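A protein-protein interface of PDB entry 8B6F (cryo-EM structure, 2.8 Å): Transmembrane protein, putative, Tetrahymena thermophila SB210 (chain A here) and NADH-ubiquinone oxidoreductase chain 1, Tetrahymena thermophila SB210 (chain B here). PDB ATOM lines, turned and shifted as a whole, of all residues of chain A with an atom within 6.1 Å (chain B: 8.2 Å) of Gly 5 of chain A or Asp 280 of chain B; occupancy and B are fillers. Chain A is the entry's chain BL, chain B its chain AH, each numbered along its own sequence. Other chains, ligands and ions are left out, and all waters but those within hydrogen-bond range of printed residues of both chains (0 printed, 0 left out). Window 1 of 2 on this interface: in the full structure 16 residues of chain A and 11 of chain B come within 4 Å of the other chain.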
ATOM      1  N   THR A   2     -15.732 -21.310 -25.273  1.00  0.00           N
ATOM      2  CA  THR A   2     -15.911 -19.866 -25.583  1.00  0.00           C
ATOM      3  C   THR A   2     -16.187 -19.669 -27.070  1.00  0.00           C
ATOM      4  O   THR A   2     -15.834 -20.511 -27.892  1.00  0.00           O
ATOM      5  CB  THR A   2     -14.675 -19.048 -25.175  1.00  0.00           C
ATOM      6  OG1 THR A   2     -13.508 -19.592 -25.802  1.00  0.00           O
ATOM      7  CG2 THR A   2     -14.490 -19.071 -23.668  1.00  0.00           C
ATOM      8  N   ASN A   3     -16.819 -18.545 -27.411  1.00  0.00           N
ATOM      9  CA  ASN A   3     -17.184 -18.294 -28.801  1.00  0.00           C
ATOM     10  C   ASN A   3     -15.950 -18.158 -29.684  1.00  0.00           C
ATOM     11  O   ASN A   3     -15.842 -18.815 -30.726  1.00  0.00           O
ATOM     12  CB  ASN A   3     -18.046 -17.035 -28.894  1.00  0.00           C
ATOM     13  CG  ASN A   3     -19.342 -17.157 -28.120  1.00  0.00           C
ATOM     14  OD1 ASN A   3     -19.532 -18.095 -27.351  1.00  0.00           O
ATOM     15  ND2 ASN A   3     -20.240 -16.201 -28.318  1.00  0.00           N
ATOM     16  N   PHE A   4     -15.003 -17.309 -29.280  1.00  0.00           N
ATOM     17  CA  PHE A   4     -13.829 -17.018 -30.089  1.00  0.00           C
ATOM     18  C   PHE A   4     -12.525 -17.522 -29.496  1.00  0.00           C
ATOM     19  O   PHE A   4     -11.554 -17.687 -30.240  1.00  0.00           O
ATOM     20  CB  PHE A   4     -13.705 -15.504 -30.317  1.00  0.00           C
ATOM     21  CG  PHE A   4     -14.907 -14.888 -30.970  1.00  0.00           C
ATOM     22  CD1 PHE A   4     -15.028 -14.866 -32.349  1.00  0.00           C
ATOM     23  CD2 PHE A   4     -15.916 -14.330 -30.205  1.00  0.00           C
ATOM     24  CE1 PHE A   4     -16.134 -14.301 -32.953  1.00  0.00           C
ATOM     25  CE2 PHE A   4     -17.023 -13.762 -30.804  1.00  0.00           C
ATOM     26  CZ  PHE A   4     -17.132 -13.748 -32.179  1.00  0.00           C
ATOM     27  N   GLY A   5     -12.472 -17.776 -28.196  1.00  0.00           N
ATOM     28  CA  GLY A   5     -11.222 -18.161 -27.584  1.00  0.00           C
ATOM     29  C   GLY A   5     -10.299 -16.964 -27.436  1.00  0.00           C
ATOM     30  O   GLY A   5     -10.696 -15.806 -27.547  1.00  0.00           O
ATOM     31  N   SER A   6      -9.037 -17.272 -27.176  1.00  0.00           N
ATOM     32  CA  SER A   6      -8.050 -16.222 -27.001  1.00  0.00           C
ATOM     33  C   SER A   6      -7.827 -15.493 -28.324  1.00  0.00           C
ATOM     34  O   SER A   6      -7.840 -16.119 -29.388  1.00  0.00           O
ATOM     35  CB  SER A   6      -6.734 -16.801 -26.489  1.00  0.00           C
ATOM     36  OG  SER A   6      -6.227 -17.769 -27.387  1.00  0.00           O
ATOM     37  N   PRO A   7      -7.619 -14.173 -28.295  1.00  0.00           N
ATOM     38  CA  PRO A   7      -7.368 -13.447 -29.547  1.00  0.00           C
ATOM     39  C   PRO A   7      -5.961 -13.620 -30.084  1.00  0.00           C
ATOM     40  O   PRO A   7      -5.743 -13.384 -31.279  1.00  0.00           O
ATOM     41  CB  PRO A   7      -7.629 -11.987 -29.157  1.00  0.00           C
ATOM     42  CG  PRO A   7      -7.257 -11.932 -27.722  1.00  0.00           C
ATOM     43  CD  PRO A   7      -7.636 -13.267 -27.132  1.00  0.00           C
ATOM     44  N   ARG A   9      -4.028 -16.461 -30.199  1.00  0.00           N
ATOM     45  CA  ARG A   9      -3.796 -17.733 -30.865  1.00  0.00           C
ATOM     46  C   ARG A   9      -5.132 -18.398 -31.158  1.00  0.00           C
ATOM     47  O   ARG A   9      -6.174 -18.016 -30.623  1.00  0.00           O
ATOM     48  CB  ARG A   9      -2.914 -18.653 -30.015  1.00  0.00           C
ATOM     49  CG  ARG A   9      -3.541 -19.023 -28.692  1.00  0.00           C
ATOM     50  CD  ARG A   9      -2.527 -19.606 -27.731  1.00  0.00           C
ATOM     51  NE  ARG A   9      -3.133 -19.890 -26.438  1.00  0.00           N
ATOM     52  CZ  ARG A   9      -3.388 -18.976 -25.512  1.00  0.00           C
ATOM     53  NH1 ARG A   9      -3.105 -17.698 -25.704  1.00  0.00           N
ATOM     54  NH2 ARG A   9      -3.947 -19.352 -24.365  1.00  0.00           N
ATOM     55  N   THR A  11      -7.279 -21.020 -30.343  1.00  0.00           N
ATOM     56  CA  THR A  11      -7.428 -21.945 -29.228  1.00  0.00           C
ATOM     57  C   THR A  11      -8.035 -23.266 -29.687  1.00  0.00           C
ATOM     58  O   THR A  11      -8.963 -23.296 -30.498  1.00  0.00           O
ATOM     59  CB  THR A  11      -8.299 -21.321 -28.136  1.00  0.00           C
ATOM     60  OG1 THR A  11      -7.633 -20.179 -27.583  1.00  0.00           O
ATOM     61  CG2 THR A  11      -8.581 -22.319 -27.018  1.00  0.00           C
ATOM     62  N   ASN A 107     -15.971  -9.270 -19.941  1.00  0.00           N
ATOM     63  CA  ASN A 107     -14.986  -9.995 -20.736  1.00  0.00           C
ATOM     64  C   ASN A 107     -14.308  -9.084 -21.749  1.00  0.00           C
ATOM     65  O   ASN A 107     -13.104  -9.211 -21.996  1.00  0.00           O
ATOM     66  CB  ASN A 107     -15.648 -11.174 -21.444  1.00  0.00           C
ATOM     67  CG  ASN A 107     -14.641 -12.194 -21.925  1.00  0.00           C
ATOM     68  OD1 ASN A 107     -13.496 -11.859 -22.217  1.00  0.00           O
ATOM     69  ND2 ASN A 107     -15.063 -13.447 -22.004  1.00  0.00           N
ATOM     70  N   ILE B 192     -20.753 -20.273 -34.084  1.00  0.00           N
ATOM     71  CA  ILE B 192     -21.321 -19.564 -32.938  1.00  0.00           C
ATOM     72  C   ILE B 192     -22.845 -19.627 -32.968  1.00  0.00           C
ATOM     73  O   ILE B 192     -23.482 -20.061 -32.003  1.00  0.00           O
ATOM     74  CB  ILE B 192     -20.813 -18.111 -32.897  1.00  0.00           C
ATOM     75  CG1 ILE B 192     -19.291 -18.096 -32.730  1.00  0.00           C
ATOM     76  CG2 ILE B 192     -21.476 -17.342 -31.758  1.00  0.00           C
ATOM     77  CD1 ILE B 192     -18.670 -16.716 -32.774  1.00  0.00           C
ATOM     78  N   LEU B 275     -25.864 -19.726 -25.145  1.00  0.00           N
ATOM     79  CA  LEU B 275     -25.231 -18.484 -25.572  1.00  0.00           C
ATOM     80  C   LEU B 275     -25.120 -17.496 -24.420  1.00  0.00           C
ATOM     81  O   LEU B 275     -24.098 -16.817 -24.274  1.00  0.00           O
ATOM     82  CB  LEU B 275     -26.019 -17.871 -26.729  1.00  0.00           C
ATOM     83  CG  LEU B 275     -25.429 -16.604 -27.351  1.00  0.00           C
ATOM     84  CD1 LEU B 275     -24.085 -16.897 -28.001  1.00  0.00           C
ATOM     85  CD2 LEU B 275     -26.394 -16.009 -28.361  1.00  0.00           C
ATOM     86  N   PHE B 276     -26.161 -17.400 -23.592  1.00  0.00           N
ATOM     87  CA  PHE B 276     -26.142 -16.427 -22.505  1.00  0.00           C
ATOM     88  C   PHE B 276     -25.021 -16.722 -21.518  1.00  0.00           C
ATOM     89  O   PHE B 276     -24.368 -15.800 -21.017  1.00  0.00           O
ATOM     90  CB  PHE B 276     -27.494 -16.412 -21.788  1.00  0.00           C
ATOM     91  CG  PHE B 276     -28.642 -15.948 -22.647  1.00  0.00           C
ATOM     92  CD1 PHE B 276     -28.424 -15.189 -23.786  1.00  0.00           C
ATOM     93  CD2 PHE B 276     -29.944 -16.264 -22.300  1.00  0.00           C
ATOM     94  CE1 PHE B 276     -29.483 -14.762 -24.565  1.00  0.00           C
ATOM     95  CE2 PHE B 276     -31.007 -15.839 -23.074  1.00  0.00           C
ATOM     96  CZ  PHE B 276     -30.776 -15.087 -24.208  1.00  0.00           C
ATOM     97  N   LEU B 277     -24.786 -17.998 -21.222  1.00  0.00           N
ATOM     98  CA  LEU B 277     -23.767 -18.378 -20.252  1.00  0.00           C
ATOM     99  C   LEU B 277     -22.363 -18.427 -20.839  1.00  0.00           C
ATOM    100  O   LEU B 277     -21.396 -18.496 -20.074  1.00  0.00           O
ATOM    101  CB  LEU B 277     -24.106 -19.742 -19.649  1.00  0.00           C
ATOM    102  CG  LEU B 277     -25.489 -19.869 -19.008  1.00  0.00           C
ATOM    103  CD1 LEU B 277     -25.713 -21.285 -18.512  1.00  0.00           C
ATOM    104  CD2 LEU B 277     -25.659 -18.874 -17.872  1.00  0.00           C
ATOM    105  N   LEU B 278     -22.223 -18.393 -22.160  1.00  0.00           N
ATOM    106  CA  LEU B 278     -20.913 -18.523 -22.777  1.00  0.00           C
ATOM    107  C   LEU B 278     -20.120 -17.224 -22.676  1.00  0.00           C
ATOM    108  O   LEU B 278     -20.671 -16.132 -22.520  1.00  0.00           O
ATOM    109  CB  LEU B 278     -21.051 -18.928 -24.245  1.00  0.00           C
ATOM    110  CG  LEU B 278     -21.267 -20.416 -24.527  1.00  0.00           C
ATOM    111  CD1 LEU B 278     -21.621 -20.631 -25.986  1.00  0.00           C
ATOM    112  CD2 LEU B 278     -20.030 -21.219 -24.164  1.00  0.00           C
ATOM    113  N   ASN B 279     -18.799 -17.364 -22.765  1.00  0.00           N
ATOM    114  CA  ASN B 279     -17.873 -16.241 -22.795  1.00  0.00           C
ATOM    115  C   ASN B 279     -17.232 -16.155 -24.173  1.00  0.00           C
ATOM    116  O   ASN B 279     -16.906 -17.178 -24.779  1.00  0.00           O
ATOM    117  CB  ASN B 279     -16.786 -16.399 -21.730  1.00  0.00           C
ATOM    118  CG  ASN B 279     -17.316 -16.225 -20.326  1.00  0.00           C
ATOM    119  OD1 ASN B 279     -17.385 -15.111 -19.809  1.00  0.00           O
ATOM    120  ND2 ASN B 279     -17.689 -17.331 -19.694  1.00  0.00           N
ATOM    121  N   ASP B 280     -17.055 -14.931 -24.668  1.00  0.00           N
ATOM    122  CA  ASP B 280     -16.518 -14.741 -26.009  1.00  0.00           C
ATOM    123  C   ASP B 280     -14.999 -14.770 -26.067  1.00  0.00           C
ATOM    124  O   ASP B 280     -14.446 -14.873 -27.167  1.00  0.00           O
ATOM    125  CB  ASP B 280     -17.024 -13.430 -26.604  1.00  0.00           C
ATOM    126  CG  ASP B 280     -18.462 -13.527 -27.055  1.00  0.00           C
ATOM    127  OD1 ASP B 280     -19.088 -14.583 -26.822  1.00  0.00           O
ATOM    128  OD2 ASP B 280     -18.960 -12.573 -27.674  1.00  0.00           O
ATOM    129  N   PHE B 281     -14.313 -14.689 -24.932  1.00  0.00           N
ATOM    130  CA  PHE B 281     -12.859 -14.716 -24.925  1.00  0.00           C
ATOM    131  C   PHE B 281     -12.387 -15.380 -23.642  1.00  0.00           C
ATOM    132  O   PHE B 281     -13.117 -15.456 -22.652  1.00  0.00           O
ATOM    133  CB  PHE B 281     -12.255 -13.308 -25.032  1.00  0.00           C
ATOM    134  CG  PHE B 281     -12.594 -12.590 -26.306  1.00  0.00           C
ATOM    135  CD1 PHE B 281     -11.966 -12.922 -27.493  1.00  0.00           C
ATOM    136  CD2 PHE B 281     -13.523 -11.562 -26.309  1.00  0.00           C
ATOM    137  CE1 PHE B 281     -12.270 -12.258 -28.664  1.00  0.00           C
ATOM    138  CE2 PHE B 281     -13.831 -10.893 -27.478  1.00  0.00           C
ATOM    139  CZ  PHE B 281     -13.203 -11.241 -28.656  1.00  0.00           C
ATOM    140  N   ASN B 282     -11.148 -15.860 -23.675  1.00  0.00           N
ATOM    141  CA  ASN B 282     -10.494 -16.421 -22.496  1.00  0.00           C
ATOM    142  C   ASN B 282      -9.070 -15.887 -22.465  1.00  0.00           C
ATOM    143  O   ASN B 282      -8.224 -16.315 -23.257  1.00  0.00           O
ATOM    144  CB  ASN B 282     -10.514 -17.950 -22.518  1.00  0.00           C
ATOM    145  CG  ASN B 282      -9.839 -18.524 -23.742  1.00  0.00           C
ATOM    146  OD1 ASN B 282      -9.717 -17.856 -24.767  1.00  0.00           O
ATOM    147  ND2 ASN B 282      -9.397 -19.771 -23.643  1.00  0.00           N
ATOM    148  N   ILE B 283      -8.812 -14.944 -21.565  1.00  0.00           N
ATOM    149  CA  ILE B 283      -7.500 -14.331 -21.406  1.00  0.00           C
ATOM    150  C   ILE B 283      -6.999 -14.653 -20.007  1.00  0.00           C
ATOM    151  O   ILE B 283      -7.701 -14.407 -19.020  1.00  0.00           O
ATOM    152  CB  ILE B 283      -7.547 -12.808 -21.626  1.00  0.00           C
ATOM    153  CG1 ILE B 283      -8.195 -12.458 -22.969  1.00  0.00           C
ATOM    154  CG2 ILE B 283      -6.151 -12.220 -21.564  1.00  0.00           C
ATOM    155  CD1 ILE B 283      -9.710 -12.382 -22.934  1.00  0.00           C
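N of Phe 4 of chain A lies within hydrogen-bond range of O of Asp 280 of chain B, at 3.3 Å. The backbone carbonyl oxygen (O) of Asn 279 of chain B is in hydrogen-bond range of the backbone NH (N) of Asn 3 of chain A. The side-chain carboxylate (OD1) of Asp 280 of chain B sits at hydrogen-bond distance from the side-chain amide nitrogen (ND2) of Asn 3 of chain A (2.5 Å). The side-chain amide nitrogen (ND2) of Asn 107 of chain A sits at hydrogen-bond distance from the backbone carbonyl oxygen (O) of Phe 281 of chain B (2.9 Å). The side-chain amide oxygen (OD1) of Asn 282 of chain B is in hydrogen-bond range of the backbone NH (N) of Ser 6 of chain A (2.6 Å).
OG of Ser 6 of chain A is in hydrogen-bond range of OG1 of Thr 11 of chain A (2.8 Å). The side-chain hydroxyl of Thr 2 of chain A is in hydrogen-bond range of the backbone NH of Gly 5 of chain A (3.2 Å). The backbone carbonyl oxygen (O) of Arg 9 of chain A sits close to the side-chain hydroxyl (OG) of Ser 6 of chain A (3.2 Å).
Among the printed residues, pairs that only touch across the chains: Gly 5 of chain A with Asn 282 of chain B (2.9 Å), Thr 2 of chain A with Asn 279 of chain B (2.9 Å), Gly 5 of chain A with Phe 281 of chain B (3.2 Å), Phe 4 of chain A with Ile 192 of chain B (3.4 Å), Asn 107 of chain A with Asn 279 of chain B (3.4 Å), Asn 3 of chain A with Leu 278 of chain B (3.6 Å), Asn 107 of chain A with Asp 280 of chain B (3.6 Å), Gly 5 of chain A with Asp 280 of chain B (3.7 Å), Asn 3 of chain A with Ile 192 of chain B (3.8 Å), Asn 107 of chain A with Ile 283 of chain B (3.9 Å), Phe 4 of chain A with Phe 281 of chain B (3.9 Å), Asn 3 of chain A with Leu 275 of chain B (3.9 Å) and Thr 2 of chain A with Phe 281 of chain B (3.998 Å).
Of the 9 printed residues of chain A, 6 touch a printed residue of chain B. Among the printed residues, no Asp or Glu carboxylate lies within 4 Å of a Lys or Arg side-chain nitrogen of the other chain.
Of the printed residues of chain B, Thr 2 of chain A touches Asn 279 (2.9 Å) and Phe 281 (3.998 Å). Of the printed residues of chain B, Phe 4 of chain A touches Ile 192, Asp 280 and Phe 281. Of chain B, only Asp 280, Phe 281 and Asn 282 come within 4 Å of Gly 5 of chain A. Printed residues of chain B within 4 Å of Ser 6 of chain A: Asn 282 (2.6 Å). Pro 7 of chain A touches none of the printed residues of chain B. Asp 280 of chain B touches just these residues of chain A: Asn 3, Phe 4, Gly 5 and Asn 107. Printed residues of chain A within 4 Å of Phe 281 of chain B: Thr 2, Phe 4, Gly 5 and Asn 107. Of the printed residues of chain A, Ile 283 of chain B touches Asn 107 (3.9 Å). The nearest residue of chain B that does not touch Gly 5 of chain A is Asn 279 of chain B (5.6 Å). The nearest printed residue of chain B that does not touch Phe 4 of chain A is Asn 279 of chain B (4.9 Å).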
